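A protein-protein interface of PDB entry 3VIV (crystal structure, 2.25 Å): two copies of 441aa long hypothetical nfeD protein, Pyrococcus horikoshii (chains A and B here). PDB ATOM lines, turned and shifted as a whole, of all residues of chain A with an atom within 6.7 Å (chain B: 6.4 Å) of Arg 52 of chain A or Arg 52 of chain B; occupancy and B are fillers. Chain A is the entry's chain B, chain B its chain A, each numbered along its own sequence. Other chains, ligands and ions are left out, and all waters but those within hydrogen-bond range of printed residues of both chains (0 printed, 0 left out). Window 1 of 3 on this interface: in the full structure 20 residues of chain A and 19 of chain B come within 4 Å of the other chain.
Arg 52 of chain A touches its own counterpart, Arg 52 of chain B. Arg 52 of chain A touches Asp 54 of chain B, and with the chains exchanged Asp 54 of chain A touches Arg 52 of chain B. Asp 54 of chain A touches Gly 111 of chain B, and with the chains exchanged Gly 111 of chain A touches Asp 54 of chain B. Leu 110 of chain A touches Met 57 of chain B, but with the chains exchanged Met 57 of chain A does not touch Leu 110 of chain B (4.8 Å). Positions printed for both chains: 18, 19, 20, 21, 50, 51, 52, 53, 54, 55, 56, 57, 83, 84, 110 and 111. Of the 8 pairs that touch across the chains among the printed residues, 7 have their exchanged pair printed and touching as well.
Of chain B, only Arg 52 (3.4 Å) and Asp 54 (3.0 Å) come within 4 Å of Arg 52 of chain A. Of chain A, only Arg 52 and Asp 54 come within 4 Å of Arg 52 of chain B. Printed residues of chain A within 4 Å of Asp 54 of chain B: Arg 52, Leu 110 and Gly 111. Of the printed residues of chain A, Leu 110 of chain B touches Asp 54 (3.2 Å). Printed residues of chain B within 4 Å of Gly 111 of chain A: Asp 54 (3.9 Å). Of the printed residues of chain B, Leu 110 of chain A touches Asp 54 and Met 57. Of the printed residues of chain A, Met 57 of chain B touches Leu 110 (3.9 Å). Thr 20 of chain A touches none of the printed residues of chain B. Ile 19 of chain B touches none of the printed residues of chain A.
O of Ile 19 of chain B is in hydrogen-bond range of N of Arg 52 of chain B, 2.8 Å away. O of Ile 19 of chain A sits at hydrogen-bond distance from N of Arg 52 of chain A (2.7 Å).
Of the 16 printed residues of chain B, 5 touch a printed residue of chain A. Hydrophobic or aromatic side chains of chain B that line the printed part of chain A: Met 57. Printed residues of chain A that touch a printed residue of chain B: Arg 52, Asp 54, Leu 110 and Gly 111. Hydrophobic or aromatic side chains of chain A within 4 Å of the printed part of chain B: Leu 110. Among the printed residues, Asp or Glu carboxylates within 4 Å of a Lys or Arg side-chain nitrogen of the other chain: Arg 52 of chain A with Asp 54 of chain B and Asp 54 of chain A with Arg 52 of chain B.
Asp 54 of chain A touches Leu 110 of chain B (CB to O, 3.2 Å). Asp 54 of chain A touches Gly 111 of chain B. Asp 54 of chain B touches Leu 110 of chain A. Met 57 of chain B touches Leu 110 of chain A (CE to CD1, 3.9 Å). Gly 111 of chain A touches Asp 54 of chain B (CA to CB, 3.9 Å).
The guanidinium group (NH1) of Arg 52 of chain B is in salt-bridge range of the side-chain carboxylate (OD2) of Asp 54 of chain A (3.1 Å). The side-chain carboxylate (OD2) of Asp 54 of chain B is in salt-bridge range of the guanidinium group (NH2) of Arg 52 of chain A (3.0 Å). The guanidinium group (NE) of Arg 52 of chain A lies close to the guanidinium group (NH2) of Arg 52 of chain B (3.5 Å).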
ATOM      1  N   GLN A  18      -1.084  15.036  31.747  1.00  0.00           N
ATOM      2  CA  GLN A  18      -0.734  16.080  30.804  1.00  0.00           C
ATOM      3  C   GLN A  18      -0.123  15.502  29.541  1.00  0.00           C
ATOM      4  O   GLN A  18       0.707  14.585  29.615  1.00  0.00           O
ATOM      5  CB  GLN A  18       0.246  17.075  31.450  1.00  0.00           C
ATOM      6  CG  GLN A  18      -0.370  17.890  32.585  1.00  0.00           C
ATOM      7  CD  GLN A  18      -0.827  19.283  32.143  1.00  0.00           C
ATOM      8  OE1 GLN A  18      -1.926  19.733  32.497  1.00  0.00           O
ATOM      9  NE2 GLN A  18       0.023  19.976  31.370  1.00  0.00           N
ATOM     10  N   ILE A  19      -0.518  16.055  28.396  1.00  0.00           N
ATOM     11  CA  ILE A  19       0.039  15.633  27.112  1.00  0.00           C
ATOM     12  C   ILE A  19       1.449  16.219  26.966  1.00  0.00           C
ATOM     13  O   ILE A  19       1.625  17.429  26.877  1.00  0.00           O
ATOM     14  CB  ILE A  19      -0.846  16.043  25.897  1.00  0.00           C
ATOM     15  CG1 ILE A  19      -2.304  15.541  26.033  1.00  0.00           C
ATOM     16  CG2 ILE A  19      -0.189  15.599  24.605  1.00  0.00           C
ATOM     17  CD1 ILE A  19      -2.500  13.994  26.060  1.00  0.00           C
ATOM     18  N   THR A  20       2.442  15.336  26.970  1.00  0.00           N
ATOM     19  CA  THR A  20       3.839  15.702  26.797  1.00  0.00           C
ATOM     20  C   THR A  20       4.464  14.665  25.871  1.00  0.00           C
ATOM     21  O   THR A  20       3.773  13.781  25.365  1.00  0.00           O
ATOM     22  CB  THR A  20       4.636  15.638  28.167  1.00  0.00           C
ATOM     23  OG1 THR A  20       4.794  14.270  28.545  1.00  0.00           O
ATOM     24  CG2 THR A  20       3.930  16.378  29.279  1.00  0.00           C
ATOM     25  N   SER A  21       5.786  14.747  25.718  1.00  0.00           N
ATOM     26  CA  SER A  21       6.580  13.803  24.931  1.00  0.00           C
ATOM     27  C   SER A  21       6.514  12.362  25.425  1.00  0.00           C
ATOM     28  O   SER A  21       6.691  11.426  24.635  1.00  0.00           O
ATOM     29  CB  SER A  21       8.035  14.254  24.932  1.00  0.00           C
ATOM     30  OG  SER A  21       8.094  15.594  24.475  1.00  0.00           O
ATOM     31  N   GLY A  50      -4.963  18.622  29.477  1.00  0.00           N
ATOM     32  CA  GLY A  50      -4.268  19.435  28.478  1.00  0.00           C
ATOM     33  C   GLY A  50      -2.812  19.047  28.314  1.00  0.00           C
ATOM     34  O   GLY A  50      -2.402  17.941  28.699  1.00  0.00           O
ATOM     35  N   GLY A  51      -2.028  19.957  27.747  1.00  0.00           N
ATOM     36  CA  GLY A  51      -0.610  19.736  27.592  1.00  0.00           C
ATOM     37  C   GLY A  51       0.039  20.524  26.481  1.00  0.00           C
ATOM     38  O   GLY A  51      -0.406  21.622  26.140  1.00  0.00           O
ATOM     39  N   ARG A  52       1.113  19.949  25.937  1.00  0.00           N
ATOM     40  CA  ARG A  52       1.998  20.626  24.999  1.00  0.00           C
ATOM     41  C   ARG A  52       1.574  20.443  23.530  1.00  0.00           C
ATOM     42  O   ARG A  52       1.256  19.325  23.092  1.00  0.00           O
ATOM     43  CB  ARG A  52       3.446  20.138  25.196  1.00  0.00           C
ATOM     44  CG  ARG A  52       4.085  20.286  26.642  1.00  0.00           C
ATOM     45  CD  ARG A  52       3.551  21.465  27.534  1.00  0.00           C
ATOM     46  NE  ARG A  52       4.033  22.793  27.148  1.00  0.00           N
ATOM     47  CZ  ARG A  52       4.330  23.785  27.998  1.00  0.00           C
ATOM     48  NH1 ARG A  52       4.237  23.624  29.311  1.00  0.00           N
ATOM     49  NH2 ARG A  52       4.742  24.947  27.528  1.00  0.00           N
ATOM     50  N   ALA A  53       1.603  21.546  22.784  1.00  0.00           N
ATOM     51  CA  ALA A  53       1.184  21.611  21.388  1.00  0.00           C
ATOM     52  C   ALA A  53       1.968  20.698  20.450  1.00  0.00           C
ATOM     53  O   ALA A  53       1.350  19.993  19.641  1.00  0.00           O
ATOM     54  CB  ALA A  53       1.217  23.045  20.884  1.00  0.00           C
ATOM     55  N   ASP A  54       3.300  20.679  20.567  1.00  0.00           N
ATOM     56  CA  ASP A  54       4.108  19.837  19.680  1.00  0.00           C
ATOM     57  C   ASP A  54       3.856  18.346  19.889  1.00  0.00           C
ATOM     58  O   ASP A  54       3.714  17.593  18.914  1.00  0.00           O
ATOM     59  CB  ASP A  54       5.608  20.205  19.649  1.00  0.00           C
ATOM     60  CG  ASP A  54       6.382  19.907  20.968  1.00  0.00           C
ATOM     61  OD1 ASP A  54       7.579  19.553  20.843  1.00  0.00           O
ATOM     62  OD2 ASP A  54       5.853  20.055  22.098  1.00  0.00           O
ATOM     63  N   ALA A  55       3.740  17.935  21.154  1.00  0.00           N
ATOM     64  CA  ALA A  55       3.491  16.525  21.459  1.00  0.00           C
ATOM     65  C   ALA A  55       2.110  16.106  20.954  1.00  0.00           C
ATOM     66  O   ALA A  55       1.937  15.006  20.460  1.00  0.00           O
ATOM     67  CB  ALA A  55       3.641  16.249  22.955  1.00  0.00           C
ATOM     68  N   MET A  56       1.145  17.007  21.077  1.00  0.00           N
ATOM     69  CA  MET A  56      -0.194  16.795  20.588  1.00  0.00           C
ATOM     70  C   MET A  56      -0.235  16.597  19.056  1.00  0.00           C
ATOM     71  O   MET A  56      -0.924  15.706  18.548  1.00  0.00           O
ATOM     72  CB  MET A  56      -1.060  17.989  20.976  1.00  0.00           C
ATOM     73  CG  MET A  56      -2.442  17.956  20.390  1.00  0.00           C
ATOM     74  SD  MET A  56      -2.453  18.878  18.850  1.00  0.00           S
ATOM     75  CE  MET A  56      -2.571  20.561  19.544  1.00  0.00           C
ATOM     76  N   MET A  57       0.479  17.453  18.344  1.00  0.00           N
ATOM     77  CA  MET A  57       0.516  17.402  16.884  1.00  0.00           C
ATOM     78  C   MET A  57       1.259  16.161  16.409  1.00  0.00           C
ATOM     79  O   MET A  57       0.858  15.535  15.429  1.00  0.00           O
ATOM     80  CB  MET A  57       1.143  18.668  16.309  1.00  0.00           C
ATOM     81  CG  MET A  57       0.254  19.878  16.461  1.00  0.00           C
ATOM     82  SD  MET A  57       1.108  21.358  15.902  1.00  0.00           S
ATOM     83  CE  MET A  57      -0.168  22.548  16.270  1.00  0.00           C
ATOM     84  N   SER A  83      -8.429  20.820  26.111  1.00  0.00           N
ATOM     85  CA  SER A  83      -7.211  21.441  25.608  1.00  0.00           C
ATOM     86  C   SER A  83      -6.576  20.497  24.569  1.00  0.00           C
ATOM     87  O   SER A  83      -7.294  20.006  23.707  1.00  0.00           O
ATOM     88  CB  SER A  83      -6.288  21.772  26.787  1.00  0.00           C
ATOM     89  OG  SER A  83      -4.991  22.143  26.358  1.00  0.00           O
ATOM     90  N   ALA A  84      -5.264  20.243  24.641  1.00  0.00           N
ATOM     91  CA  ALA A  84      -4.584  19.352  23.678  1.00  0.00           C
ATOM     92  C   ALA A  84      -5.324  18.033  23.437  1.00  0.00           C
ATOM     93  O   ALA A  84      -5.298  17.489  22.324  1.00  0.00           O
ATOM     94  CB  ALA A  84      -3.155  19.065  24.110  1.00  0.00           C
ATOM     95  N   LEU A 110      -0.159  31.116  26.351  1.00  0.00           N
ATOM     96  CA  LEU A 110       1.277  30.878  26.405  1.00  0.00           C
ATOM     97  C   LEU A 110       1.603  30.037  27.630  1.00  0.00           C
ATOM     98  O   LEU A 110       2.541  29.252  27.603  1.00  0.00           O
ATOM     99  CB  LEU A 110       2.072  32.180  26.375  1.00  0.00           C
ATOM    100  CG  LEU A 110       2.201  32.859  25.006  1.00  0.00           C
ATOM    101  CD1 LEU A 110       3.115  34.077  25.082  1.00  0.00           C
ATOM    102  CD2 LEU A 110       2.722  31.891  23.962  1.00  0.00           C
ATOM    103  N   GLY A 111       0.795  30.176  28.681  1.00  0.00           N
ATOM    104  CA  GLY A 111       0.901  29.333  29.873  1.00  0.00           C
ATOM    105  C   GLY A 111       0.400  30.019  31.130  1.00  0.00           C
ATOM    106  O   GLY A 111      -0.159  31.105  31.067  1.00  0.00           O
ATOM    107  N   GLN B  18      17.110  21.255  30.633  1.00  0.00           N
ATOM    108  CA  GLN B  18      15.983  21.925  30.026  1.00  0.00           C
ATOM    109  C   GLN B  18      15.289  22.794  31.064  1.00  0.00           C
ATOM    110  O   GLN B  18      15.145  22.387  32.212  1.00  0.00           O
ATOM    111  CB  GLN B  18      14.980  20.925  29.439  1.00  0.00           C
ATOM    112  CG  GLN B  18      15.514  20.066  28.282  1.00  0.00           C
ATOM    113  CD  GLN B  18      15.679  20.847  26.976  1.00  0.00           C
ATOM    114  OE1 GLN B  18      16.793  20.978  26.462  1.00  0.00           O
ATOM    115  NE2 GLN B  18      14.567  21.356  26.430  1.00  0.00           N
ATOM    116  N   ILE B  19      14.895  23.994  30.629  1.00  0.00           N
ATOM    117  CA  ILE B  19      14.011  24.884  31.371  1.00  0.00           C
ATOM    118  C   ILE B  19      12.562  24.450  31.247  1.00  0.00           C
ATOM    119  O   ILE B  19      11.922  24.646  30.191  1.00  0.00           O
ATOM    120  CB  ILE B  19      14.100  26.347  30.870  1.00  0.00           C
ATOM    121  CG1 ILE B  19      15.551  26.832  30.837  1.00  0.00           C
ATOM    122  CG2 ILE B  19      13.237  27.258  31.765  1.00  0.00           C
ATOM    123  CD1 ILE B  19      16.232  26.812  32.242  1.00  0.00           C
ATOM    124  N   THR B  20      12.045  23.883  32.335  1.00  0.00           N
ATOM    125  CA  THR B  20      10.668  23.403  32.410  1.00  0.00           C
ATOM    126  C   THR B  20      10.007  24.015  33.639  1.00  0.00           C
ATOM    127  O   THR B  20      10.653  24.762  34.390  1.00  0.00           O
ATOM    128  CB  THR B  20      10.620  21.850  32.605  1.00  0.00           C
ATOM    129  OG1 THR B  20      11.281  21.513  33.838  1.00  0.00           O
ATOM    130  CG2 THR B  20      11.293  21.106  31.434  1.00  0.00           C
ATOM    131  N   SER B  21       8.744  23.650  33.868  1.00  0.00           N
ATOM    132  CA  SER B  21       8.008  24.058  35.056  1.00  0.00           C
ATOM    133  C   SER B  21       8.776  23.707  36.303  1.00  0.00           C
ATOM    134  O   SER B  21       8.720  24.426  37.306  1.00  0.00           O
ATOM    135  CB  SER B  21       6.669  23.338  35.129  1.00  0.00           C
ATOM    136  OG  SER B  21       5.950  23.577  33.934  1.00  0.00           O
ATOM    137  N   GLY B  50      18.157  24.583  26.238  1.00  0.00           N
ATOM    138  CA  GLY B  50      16.807  24.846  25.749  1.00  0.00           C
ATOM    139  C   GLY B  50      15.728  24.805  26.819  1.00  0.00           C
ATOM    140  O   GLY B  50      16.013  24.575  28.002  1.00  0.00           O
ATOM    141  N   GLY B  51      14.485  25.016  26.384  1.00  0.00           N
ATOM    142  CA  GLY B  51      13.339  24.905  27.253  1.00  0.00           C
ATOM    143  C   GLY B  51      12.051  25.563  26.789  1.00  0.00           C
ATOM    144  O   GLY B  51      11.902  25.958  25.635  1.00  0.00           O
ATOM    145  N   ARG B  52      11.113  25.668  27.718  1.00  0.00           N
ATOM    146  CA  ARG B  52       9.780  26.143  27.392  1.00  0.00           C
ATOM    147  C   ARG B  52       9.613  27.649  27.688  1.00  0.00           C
ATOM    148  O   ARG B  52      10.136  28.178  28.689  1.00  0.00           O
ATOM    149  CB  ARG B  52       8.763  25.312  28.149  1.00  0.00           C
ATOM    150  CG  ARG B  52       8.816  23.807  27.816  1.00  0.00           C
ATOM    151  CD  ARG B  52       7.738  23.434  26.775  1.00  0.00           C
ATOM    152  NE  ARG B  52       8.046  22.180  26.087  1.00  0.00           N
ATOM    153  CZ  ARG B  52       7.364  21.705  25.043  1.00  0.00           C
ATOM    154  NH1 ARG B  52       7.726  20.555  24.475  1.00  0.00           N
ATOM    155  NH2 ARG B  52       6.320  22.378  24.575  1.00  0.00           N
ATOM    156  N   ALA B  53       8.878  28.318  26.806  1.00  0.00           N
ATOM    157  CA  ALA B  53       8.652  29.752  26.865  1.00  0.00           C
ATOM    158  C   ALA B  53       7.920  30.135  28.153  1.00  0.00           C
ATOM    159  O   ALA B  53       8.342  31.056  28.857  1.00  0.00           O
ATOM    160  CB  ALA B  53       7.842  30.199  25.626  1.00  0.00           C
ATOM    161  N   ASP B  54       6.840  29.423  28.466  1.00  0.00           N
ATOM    162  CA  ASP B  54       6.086  29.698  29.700  1.00  0.00           C
ATOM    163  C   ASP B  54       6.925  29.620  30.992  1.00  0.00           C
ATOM    164  O   ASP B  54       6.910  30.547  31.809  1.00  0.00           O
ATOM    165  CB  ASP B  54       4.801  28.856  29.785  1.00  0.00           C
ATOM    166  CG  ASP B  54       5.061  27.354  29.921  1.00  0.00           C
ATOM    167  OD1 ASP B  54       4.181  26.678  30.465  1.00  0.00           O
ATOM    168  OD2 ASP B  54       6.112  26.840  29.480  1.00  0.00           O
ATOM    169  N   ALA B  55       7.695  28.548  31.168  1.00  0.00           N
ATOM    170  CA  ALA B  55       8.541  28.458  32.352  1.00  0.00           C
ATOM    171  C   ALA B  55       9.585  29.583  32.396  1.00  0.00           C
ATOM    172  O   ALA B  55       9.845  30.149  33.459  1.00  0.00           O
ATOM    173  CB  ALA B  55       9.189  27.083  32.484  1.00  0.00           C
ATOM    174  N   MET B  56      10.170  29.881  31.243  1.00  0.00           N
ATOM    175  CA  MET B  56      11.145  30.944  31.076  1.00  0.00           C
ATOM    176  C   MET B  56      10.564  32.308  31.493  1.00  0.00           C
ATOM    177  O   MET B  56      11.199  33.045  32.245  1.00  0.00           O
ATOM    178  CB  MET B  56      11.589  31.017  29.608  1.00  0.00           C
ATOM    179  CG  MET B  56      12.470  32.238  29.256  1.00  0.00           C
ATOM    180  SD  MET B  56      11.505  33.674  28.658  1.00  0.00           S
ATOM    181  CE  MET B  56      11.003  33.022  27.038  1.00  0.00           C
ATOM    182  N   MET B  57       9.371  32.633  30.982  1.00  0.00           N
ATOM    183  CA  MET B  57       8.713  33.894  31.340  1.00  0.00           C
ATOM    184  C   MET B  57       8.397  33.987  32.827  1.00  0.00           C
ATOM    185  O   MET B  57       8.527  35.071  33.415  1.00  0.00           O
ATOM    186  CB  MET B  57       7.468  34.159  30.483  1.00  0.00           C
ATOM    187  CG  MET B  57       7.797  34.302  29.008  1.00  0.00           C
ATOM    188  SD  MET B  57       6.341  34.640  28.009  1.00  0.00           S
ATOM    189  CE  MET B  57       6.698  33.696  26.558  1.00  0.00           C
ATOM    190  N   SER B  83      18.801  29.554  23.937  1.00  0.00           N
ATOM    191  CA  SER B  83      17.362  29.372  23.901  1.00  0.00           C
ATOM    192  C   SER B  83      16.747  30.047  25.144  1.00  0.00           C
ATOM    193  O   SER B  83      17.059  31.203  25.392  1.00  0.00           O
ATOM    194  CB  SER B  83      17.057  27.873  23.728  1.00  0.00           C
ATOM    195  OG  SER B  83      15.725  27.517  24.071  1.00  0.00           O
ATOM    196  N   ALA B  84      15.928  29.353  25.939  1.00  0.00           N
ATOM    197  CA  ALA B  84      15.281  29.956  27.125  1.00  0.00           C
ATOM    198  C   ALA B  84      16.235  30.561  28.118  1.00  0.00           C
ATOM    199  O   ALA B  84      15.884  31.544  28.777  1.00  0.00           O
ATOM    200  CB  ALA B  84      14.345  28.970  27.848  1.00  0.00           C
ATOM    201  N   LEU B 110       7.646  26.059  17.543  1.00  0.00           N
ATOM    202  CA  LEU B 110       6.542  25.278  18.055  1.00  0.00           C
ATOM    203  C   LEU B 110       7.038  23.932  18.574  1.00  0.00           C
ATOM    204  O   LEU B 110       6.353  23.285  19.370  1.00  0.00           O
ATOM    205  CB  LEU B 110       5.417  25.124  17.011  1.00  0.00           C
ATOM    206  CG  LEU B 110       4.163  25.992  17.229  1.00  0.00           C
ATOM    207  CD1 LEU B 110       3.216  25.947  16.021  1.00  0.00           C
ATOM    208  CD2 LEU B 110       3.413  25.595  18.517  1.00  0.00           C
ATOM    209  N   GLY B 111       8.225  23.514  18.135  1.00  0.00           N
ATOM    210  CA  GLY B 111       8.887  22.340  18.712  1.00  0.00           C
ATOM    211  C   GLY B 111       9.448  21.377  17.679  1.00  0.00           C
ATOM    212  O   GLY B 111      10.005  21.805  16.669  1.00  0.00           O
